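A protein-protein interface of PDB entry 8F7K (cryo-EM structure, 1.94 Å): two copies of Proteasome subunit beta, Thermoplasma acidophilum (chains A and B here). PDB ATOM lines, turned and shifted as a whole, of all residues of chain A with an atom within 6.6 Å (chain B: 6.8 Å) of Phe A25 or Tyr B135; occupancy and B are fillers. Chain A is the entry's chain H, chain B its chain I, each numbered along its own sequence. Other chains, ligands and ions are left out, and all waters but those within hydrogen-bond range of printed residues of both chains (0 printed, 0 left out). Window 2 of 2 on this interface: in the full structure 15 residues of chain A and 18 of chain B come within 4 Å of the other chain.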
ATOM      1  N   VAL A  20     -21.526 -31.373  -8.514  1.00  0.00           N
ATOM      2  CA  VAL A  20     -20.571 -32.460  -8.881  1.00  0.00           C
ATOM      3  C   VAL A  20     -19.809 -32.933  -7.637  1.00  0.00           C
ATOM      4  O   VAL A  20     -19.178 -32.110  -6.991  1.00  0.00           O
ATOM      5  CB  VAL A  20     -19.631 -32.066 -10.039  1.00  0.00           C
ATOM      6  CG1 VAL A  20     -18.682 -33.191 -10.420  1.00  0.00           C
ATOM      7  CG2 VAL A  20     -20.382 -31.541 -11.249  1.00  0.00           C
ATOM      8  N   THR A  21     -19.880 -34.211  -7.329  1.00  0.00           N
ATOM      9  CA  THR A  21     -19.234 -34.791  -6.128  1.00  0.00           C
ATOM     10  C   THR A  21     -17.945 -35.506  -6.549  1.00  0.00           C
ATOM     11  O   THR A  21     -18.046 -36.628  -7.011  1.00  0.00           O
ATOM     12  CB  THR A  21     -20.211 -35.658  -5.333  1.00  0.00           C
ATOM     13  OG1 THR A  21     -20.719 -36.693  -6.171  1.00  0.00           O
ATOM     14  CG2 THR A  21     -21.369 -34.869  -4.764  1.00  0.00           C
ATOM     15  N   MET A  22     -16.802 -34.831  -6.500  1.00  0.00           N
ATOM     16  CA  MET A  22     -15.458 -35.384  -6.875  1.00  0.00           C
ATOM     17  C   MET A  22     -14.639 -35.579  -5.582  1.00  0.00           C
ATOM     18  O   MET A  22     -14.608 -34.633  -4.790  1.00  0.00           O
ATOM     19  CB  MET A  22     -14.812 -34.388  -7.852  1.00  0.00           C
ATOM     20  CG  MET A  22     -14.002 -34.911  -9.021  1.00  0.00           C
ATOM     21  SD  MET A  22     -13.004 -33.541  -9.712  1.00  0.00           S
ATOM     22  CE  MET A  22     -13.707 -33.364 -11.351  1.00  0.00           C
ATOM     23  N   GLU A  23     -14.093 -36.774  -5.308  1.00  0.00           N
ATOM     24  CA  GLU A  23     -13.301 -37.131  -4.079  1.00  0.00           C
ATOM     25  C   GLU A  23     -14.171 -37.148  -2.816  1.00  0.00           C
ATOM     26  O   GLU A  23     -13.639 -36.799  -1.759  1.00  0.00           O
ATOM     27  CB  GLU A  23     -12.032 -36.295  -3.872  1.00  0.00           C
ATOM     28  CG  GLU A  23     -11.241 -36.031  -5.135  1.00  0.00           C
ATOM     29  CD  GLU A  23     -11.483 -34.646  -5.705  1.00  0.00           C
ATOM     30  OE1 GLU A  23     -11.229 -34.445  -6.908  1.00  0.00           O
ATOM     31  OE2 GLU A  23     -11.935 -33.778  -4.943  1.00  0.00           O
ATOM     32  N   ASN A  24     -15.448 -37.511  -2.929  1.00  0.00           N
ATOM     33  CA  ASN A  24     -16.335 -37.683  -1.749  1.00  0.00           C
ATOM     34  C   ASN A  24     -16.689 -36.379  -1.023  1.00  0.00           C
ATOM     35  O   ASN A  24     -16.961 -36.451   0.172  1.00  0.00           O
ATOM     36  CB  ASN A  24     -15.760 -38.757  -0.814  1.00  0.00           C
ATOM     37  CG  ASN A  24     -15.818 -40.129  -1.446  1.00  0.00           C
ATOM     38  OD1 ASN A  24     -14.886 -40.540  -2.132  1.00  0.00           O
ATOM     39  ND2 ASN A  24     -16.926 -40.824  -1.253  1.00  0.00           N
ATOM     40  N   PHE A  25     -16.687 -35.244  -1.700  1.00  0.00           N
ATOM     41  CA  PHE A  25     -17.162 -33.978  -1.092  1.00  0.00           C
ATOM     42  C   PHE A  25     -17.767 -33.161  -2.242  1.00  0.00           C
ATOM     43  O   PHE A  25     -17.666 -33.598  -3.375  1.00  0.00           O
ATOM     44  CB  PHE A  25     -16.018 -33.300  -0.327  1.00  0.00           C
ATOM     45  CG  PHE A  25     -15.063 -32.484  -1.149  1.00  0.00           C
ATOM     46  CD1 PHE A  25     -14.028 -33.090  -1.840  1.00  0.00           C
ATOM     47  CD2 PHE A  25     -15.194 -31.109  -1.227  1.00  0.00           C
ATOM     48  CE1 PHE A  25     -13.151 -32.335  -2.601  1.00  0.00           C
ATOM     49  CE2 PHE A  25     -14.311 -30.355  -1.977  1.00  0.00           C
ATOM     50  CZ  PHE A  25     -13.294 -30.969  -2.666  1.00  0.00           C
ATOM     51  N   ILE A  26     -18.358 -32.019  -1.953  1.00  0.00           N
ATOM     52  CA  ILE A  26     -18.899 -31.167  -3.007  1.00  0.00           C
ATOM     53  C   ILE A  26     -17.802 -30.248  -3.526  1.00  0.00           C
ATOM     54  O   ILE A  26     -17.588 -29.155  -2.992  1.00  0.00           O
ATOM     55  CB  ILE A  26     -20.103 -30.350  -2.501  1.00  0.00           C
ATOM     56  CG1 ILE A  26     -21.122 -31.260  -1.811  1.00  0.00           C
ATOM     57  CG2 ILE A  26     -20.756 -29.595  -3.650  1.00  0.00           C
ATOM     58  CD1 ILE A  26     -22.254 -30.508  -1.148  1.00  0.00           C
ATOM     59  N   MET A  27     -17.099 -30.682  -4.572  1.00  0.00           N
ATOM     60  CA  MET A  27     -15.995 -29.892  -5.105  1.00  0.00           C
ATOM     61  C   MET A  27     -16.452 -28.831  -6.099  1.00  0.00           C
ATOM     62  O   MET A  27     -15.826 -27.769  -6.186  1.00  0.00           O
ATOM     63  CB  MET A  27     -14.962 -30.808  -5.765  1.00  0.00           C
ATOM     64  CG  MET A  27     -13.667 -30.113  -6.158  1.00  0.00           C
ATOM     65  SD  MET A  27     -12.355 -31.258  -6.624  1.00  0.00           S
ATOM     66  CE  MET A  27     -11.019 -30.121  -6.980  1.00  0.00           C
ATOM     67  N   HIS A  28     -17.525 -29.086  -6.843  1.00  0.00           N
ATOM     68  CA  HIS A  28     -17.999 -28.151  -7.854  1.00  0.00           C
ATOM     69  C   HIS A  28     -19.495 -27.942  -7.690  1.00  0.00           C
ATOM     70  O   HIS A  28     -20.250 -28.911  -7.565  1.00  0.00           O
ATOM     71  CB  HIS A  28     -17.638 -28.636  -9.262  1.00  0.00           C
ATOM     72  CG  HIS A  28     -16.172 -28.875  -9.458  1.00  0.00           C
ATOM     73  ND1 HIS A  28     -15.629 -30.139  -9.539  1.00  0.00           N
ATOM     74  CD2 HIS A  28     -15.137 -28.012  -9.587  1.00  0.00           C
ATOM     75  CE1 HIS A  28     -14.323 -30.045  -9.707  1.00  0.00           C
ATOM     76  NE2 HIS A  28     -13.999 -28.765  -9.738  1.00  0.00           N
ATOM     77  N   LEU B 100      -4.722 -29.578 -11.666  1.00  0.00           N
ATOM     78  CA  LEU B 100      -5.324 -28.261 -11.825  1.00  0.00           C
ATOM     79  C   LEU B 100      -4.619 -27.535 -12.959  1.00  0.00           C
ATOM     80  O   LEU B 100      -3.385 -27.524 -13.020  1.00  0.00           O
ATOM     81  CB  LEU B 100      -5.227 -27.435 -10.539  1.00  0.00           C
ATOM     82  CG  LEU B 100      -6.021 -27.907  -9.320  1.00  0.00           C
ATOM     83  CD1 LEU B 100      -5.819 -26.950  -8.155  1.00  0.00           C
ATOM     84  CD2 LEU B 100      -7.495 -28.040  -9.658  1.00  0.00           C
ATOM     85  N   SER B 112     -10.282 -28.237 -13.057  1.00  0.00           N
ATOM     86  CA  SER B 112      -9.943 -29.377 -12.217  1.00  0.00           C
ATOM     87  C   SER B 112     -10.177 -30.657 -13.005  1.00  0.00           C
ATOM     88  O   SER B 112     -11.264 -30.861 -13.554  1.00  0.00           O
ATOM     89  CB  SER B 112     -10.777 -29.382 -10.935  1.00  0.00           C
ATOM     90  OG  SER B 112     -10.514 -30.539 -10.165  1.00  0.00           O
ATOM     91  N   ASP B 122     -14.068 -23.987 -12.638  1.00  0.00           N
ATOM     92  CA  ASP B 122     -14.553 -23.420 -11.389  1.00  0.00           C
ATOM     93  C   ASP B 122     -13.808 -22.125 -11.106  1.00  0.00           C
ATOM     94  O   ASP B 122     -12.730 -21.873 -11.650  1.00  0.00           O
ATOM     95  CB  ASP B 122     -14.386 -24.408 -10.228  1.00  0.00           C
ATOM     96  CG  ASP B 122     -15.356 -24.148  -9.093  1.00  0.00           C
ATOM     97  OD1 ASP B 122     -15.666 -22.969  -8.826  1.00  0.00           O
ATOM     98  OD2 ASP B 122     -15.814 -25.128  -8.470  1.00  0.00           O
ATOM     99  N   TYR B 124     -12.548 -21.341  -8.172  1.00  0.00           N
ATOM    100  CA  TYR B 124     -11.362 -21.773  -7.446  1.00  0.00           C
ATOM    101  C   TYR B 124     -11.471 -23.268  -7.187  1.00  0.00           C
ATOM    102  O   TYR B 124     -12.563 -23.841  -7.203  1.00  0.00           O
ATOM    103  CB  TYR B 124     -11.175 -20.995  -6.135  1.00  0.00           C
ATOM    104  CG  TYR B 124     -12.340 -21.062  -5.167  1.00  0.00           C
ATOM    105  CD1 TYR B 124     -12.525 -22.166  -4.344  1.00  0.00           C
ATOM    106  CD2 TYR B 124     -13.239 -20.009  -5.059  1.00  0.00           C
ATOM    107  CE1 TYR B 124     -13.578 -22.227  -3.454  1.00  0.00           C
ATOM    108  CE2 TYR B 124     -14.296 -20.061  -4.168  1.00  0.00           C
ATOM    109  CZ  TYR B 124     -14.462 -21.173  -3.370  1.00  0.00           C
ATOM    110  OH  TYR B 124     -15.511 -21.232  -2.483  1.00  0.00           O
ATOM    111  N   ALA B 125     -10.320 -23.892  -6.949  1.00  0.00           N
ATOM    112  CA  ALA B 125     -10.273 -25.328  -6.704  1.00  0.00           C
ATOM    113  C   ALA B 125      -9.014 -25.660  -5.919  1.00  0.00           C
ATOM    114  O   ALA B 125      -8.055 -24.884  -5.885  1.00  0.00           O
ATOM    115  CB  ALA B 125     -10.320 -26.124  -8.013  1.00  0.00           C
ATOM    116  N   SER B 126      -9.033 -26.831  -5.285  1.00  0.00           N
ATOM    117  CA  SER B 126      -7.905 -27.302  -4.496  1.00  0.00           C
ATOM    118  C   SER B 126      -7.834 -28.819  -4.585  1.00  0.00           C
ATOM    119  O   SER B 126      -8.867 -29.494  -4.599  1.00  0.00           O
ATOM    120  CB  SER B 126      -8.026 -26.858  -3.032  1.00  0.00           C
ATOM    121  OG  SER B 126      -6.902 -27.270  -2.275  1.00  0.00           O
ATOM    122  N   THR B 127      -6.613 -29.347  -4.640  1.00  0.00           N
ATOM    123  CA  THR B 127      -6.384 -30.782  -4.739  1.00  0.00           C
ATOM    124  C   THR B 127      -5.393 -31.219  -3.671  1.00  0.00           C
ATOM    125  O   THR B 127      -4.677 -30.404  -3.084  1.00  0.00           O
ATOM    126  CB  THR B 127      -5.859 -31.186  -6.126  1.00  0.00           C
ATOM    127  OG1 THR B 127      -4.619 -30.518  -6.386  1.00  0.00           O
ATOM    128  CG2 THR B 127      -6.864 -30.829  -7.211  1.00  0.00           C
ATOM    129  N   GLY B 130      -4.649 -32.114   1.705  1.00  0.00           N
ATOM    130  CA  GLY B 130      -4.945 -30.904   2.438  1.00  0.00           C
ATOM    131  C   GLY B 130      -6.023 -30.030   1.841  1.00  0.00           C
ATOM    132  O   GLY B 130      -6.302 -28.953   2.379  1.00  0.00           O
ATOM    133  N   SER B 131      -6.638 -30.460   0.739  1.00  0.00           N
ATOM    134  CA  SER B 131      -7.647 -29.636   0.078  1.00  0.00           C
ATOM    135  C   SER B 131      -8.857 -29.295   0.949  1.00  0.00           C
ATOM    136  O   SER B 131      -9.302 -28.135   0.891  1.00  0.00           O
ATOM    137  CB  SER B 131      -8.092 -30.310  -1.229  1.00  0.00           C
ATOM    138  OG  SER B 131      -8.459 -31.662  -1.033  1.00  0.00           O
ATOM    139  N   PRO B 132      -9.443 -30.207   1.743  1.00  0.00           N
ATOM    140  CA  PRO B 132     -10.629 -29.809   2.524  1.00  0.00           C
ATOM    141  C   PRO B 132     -10.369 -28.661   3.486  1.00  0.00           C
ATOM    142  O   PRO B 132     -11.265 -27.841   3.719  1.00  0.00           O
ATOM    143  CB  PRO B 132     -11.011 -31.101   3.264  1.00  0.00           C
ATOM    144  CG  PRO B 132      -9.772 -31.911   3.284  1.00  0.00           C
ATOM    145  CD  PRO B 132      -9.100 -31.622   1.984  1.00  0.00           C
ATOM    146  N   PHE B 133      -9.165 -28.578   4.054  1.00  0.00           N
ATOM    147  CA  PHE B 133      -8.834 -27.446   4.914  1.00  0.00           C
ATOM    148  C   PHE B 133      -8.763 -26.152   4.112  1.00  0.00           C
ATOM    149  O   PHE B 133      -9.146 -25.084   4.606  1.00  0.00           O
ATOM    150  CB  PHE B 133      -7.517 -27.708   5.642  1.00  0.00           C
ATOM    151  CG  PHE B 133      -7.485 -29.015   6.384  1.00  0.00           C
ATOM    152  CD1 PHE B 133      -8.170 -29.164   7.578  1.00  0.00           C
ATOM    153  CD2 PHE B 133      -6.772 -30.093   5.886  1.00  0.00           C
ATOM    154  CE1 PHE B 133      -8.146 -30.365   8.262  1.00  0.00           C
ATOM    155  CE2 PHE B 133      -6.744 -31.296   6.565  1.00  0.00           C
ATOM    156  CZ  PHE B 133      -7.432 -31.431   7.755  1.00  0.00           C
ATOM    157  N   VAL B 134      -8.263 -26.227   2.876  1.00  0.00           N
ATOM    158  CA  VAL B 134      -8.213 -25.047   2.015  1.00  0.00           C
ATOM    159  C   VAL B 134      -9.619 -24.574   1.670  1.00  0.00           C
ATOM    160  O   VAL B 134      -9.906 -23.371   1.684  1.00  0.00           O
ATOM    161  CB  VAL B 134      -7.389 -25.346   0.750  1.00  0.00           C
ATOM    162  CG1 VAL B 134      -7.459 -24.181  -0.225  1.00  0.00           C
ATOM    163  CG2 VAL B 134      -5.947 -25.648   1.119  1.00  0.00           C
ATOM    164  N   TYR B 135     -10.519 -25.512   1.359  1.00  0.00           N
ATOM    165  CA  TYR B 135     -11.880 -25.137   0.988  1.00  0.00           C
ATOM    166  C   TYR B 135     -12.593 -24.424   2.130  1.00  0.00           C
ATOM    167  O   TYR B 135     -13.424 -23.541   1.896  1.00  0.00           O
ATOM    168  CB  TYR B 135     -12.669 -26.370   0.549  1.00  0.00           C
ATOM    169  CG  TYR B 135     -12.470 -26.733  -0.905  1.00  0.00           C
ATOM    170  CD1 TYR B 135     -13.160 -26.062  -1.905  1.00  0.00           C
ATOM    171  CD2 TYR B 135     -11.595 -27.746  -1.277  1.00  0.00           C
ATOM    172  CE1 TYR B 135     -12.984 -26.388  -3.237  1.00  0.00           C
ATOM    173  CE2 TYR B 135     -11.412 -28.077  -2.605  1.00  0.00           C
ATOM    174  CZ  TYR B 135     -12.108 -27.396  -3.581  1.00  0.00           C
ATOM    175  OH  TYR B 135     -11.931 -27.723  -4.904  1.00  0.00           O
ATOM    176  N   GLY B 136     -12.286 -24.799   3.373  1.00  0.00           N
ATOM    177  CA  GLY B 136     -12.862 -24.090   4.505  1.00  0.00           C
ATOM    178  C   GLY B 136     -12.436 -22.636   4.553  1.00  0.00           C
ATOM    179  O   GLY B 136     -13.246 -21.745   4.810  1.00  0.00           O
ATOM    180  N   VAL B 137     -11.151 -22.378   4.302  1.00  0.00           N
ATOM    181  CA  VAL B 137     -10.650 -21.006   4.288  1.00  0.00           C
ATOM    182  C   VAL B 137     -11.245 -20.230   3.119  1.00  0.00           C
ATOM    183  O   VAL B 137     -11.664 -19.076   3.268  1.00  0.00           O
ATOM    184  CB  VAL B 137      -9.111 -20.999   4.252  1.00  0.00           C
ATOM    185  CG1 VAL B 137      -8.581 -19.574   4.197  1.00  0.00           C
ATOM    186  CG2 VAL B 137      -8.547 -21.736   5.458  1.00  0.00           C
ATOM    187  N   LEU B 138     -11.288 -20.849   1.936  1.00  0.00           N
ATOM    188  CA  LEU B 138     -11.791 -20.156   0.754  1.00  0.00           C
ATOM    189  C   LEU B 138     -13.285 -19.867   0.864  1.00  0.00           C
ATOM    190  O   LEU B 138     -13.746 -18.804   0.437  1.00  0.00           O
ATOM    191  CB  LEU B 138     -11.491 -20.975  -0.501  1.00  0.00           C
ATOM    192  CG  LEU B 138     -10.008 -21.161  -0.829  1.00  0.00           C
ATOM    193  CD1 LEU B 138      -9.830 -21.994  -2.087  1.00  0.00           C
ATOM    194  CD2 LEU B 138      -9.315 -19.814  -0.968  1.00  0.00           C
ATOM    195  N   GLU B 139     -14.056 -20.798   1.430  1.00  0.00           N
ATOM    196  CA  GLU B 139     -15.494 -20.583   1.559  1.00  0.00           C
ATOM    197  C   GLU B 139     -15.801 -19.361   2.417  1.00  0.00           C
ATOM    198  O   GLU B 139     -16.752 -18.623   2.139  1.00  0.00           O
ATOM    199  CB  GLU B 139     -16.166 -21.826   2.146  1.00  0.00           C
ATOM    200  CG  GLU B 139     -16.511 -22.897   1.124  1.00  0.00           C
ATOM    201  CD  GLU B 139     -17.703 -22.524   0.261  1.00  0.00           C
ATOM    202  OE1 GLU B 139     -18.419 -21.564   0.611  1.00  0.00           O
ATOM    203  OE2 GLU B 139     -17.924 -23.192  -0.770  1.00  0.00           O
ATOM    204  N   SER B 140     -15.004 -19.130   3.459  1.00  0.00           N
ATOM    205  CA  SER B 140     -15.309 -18.060   4.399  1.00  0.00           C
ATOM    206  C   SER B 140     -14.651 -16.735   4.028  1.00  0.00           C
ATOM    207  O   SER B 140     -15.093 -15.683   4.503  1.00  0.00           O
ATOM    208  CB  SER B 140     -14.886 -18.470   5.811  1.00  0.00           C
ATOM    209  OG  SER B 140     -13.499 -18.750   5.869  1.00  0.00           O
ATOM    210  N   ALA B 158      -4.477 -20.032   3.288  1.00  0.00           N
ATOM    211  CA  ALA B 158      -5.175 -21.300   3.098  1.00  0.00           C
ATOM    212  C   ALA B 158      -4.212 -22.479   3.161  1.00  0.00           C
ATOM    213  O   ALA B 158      -4.500 -23.496   3.801  1.00  0.00           O
ATOM    214  CB  ALA B 158      -5.929 -21.286   1.768  1.00  0.00           C
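The side-chain carboxylate (OD2) of Asp B122 sits close to the backbone carbonyl oxygen (O) of Met A27, 3.5 Å away.
O of His A28 sits at hydrogen-bond distance from N of Val A20 (2.9 Å). The backbone NH (N) of Ser B126 sits at hydrogen-bond distance from the side-chain hydroxyl (OH) of Tyr B135 (3.1 Å). The backbone NH (N) of Met A27 lies within hydrogen-bond range of the backbone carbonyl oxygen (O) of Val A20 (3.5 Å).
Among the printed residues, merely in contact across the chains: Met A22 with Ser B112, Phe A25 with Tyr B135, Met A27 with Ser B112, Met A27 with Ser B126, Met A27 with Tyr B135, His A28 with Ser B112 and His A28 with Asp B122.
Printed residues of chain B within 4 Å of Phe A25: Tyr B135 (3.5 Å). Of chain A, only Phe A25 and Met A27 come within 4 Å of Tyr B135. Printed residues of chain A within 4 Å of Asp B122: Met A27 (3.5 Å) and His A28 (3.2 Å). Printed residues of chain B within 4 Å of His A28: Ser B112 and Asp B122. Printed residues of chain B within 4 Å of Met A22: Ser B112 (3.9 Å). Of the printed residues of chain A, Ser B126 touches Met A27 (3.3 Å). Gly B130 touches none of the printed residues of chain A. The nearest residue of chain B that does not touch Phe A25 is Ser B131 (5.0 Å).
Hydrophobic or aromatic side chains of chain A that line the printed part of chain B: Met A22, Phe A25, Met A27 and His A28. Among the printed residues, no Asp or Glu carboxylate lies within 4 Å of a Lys or Arg side-chain nitrogen of the other chain.
No position is printed for both chains. Of the 8 pairs that touch across the chains among the printed residues, none has its exchanged pair printed and touching as well.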
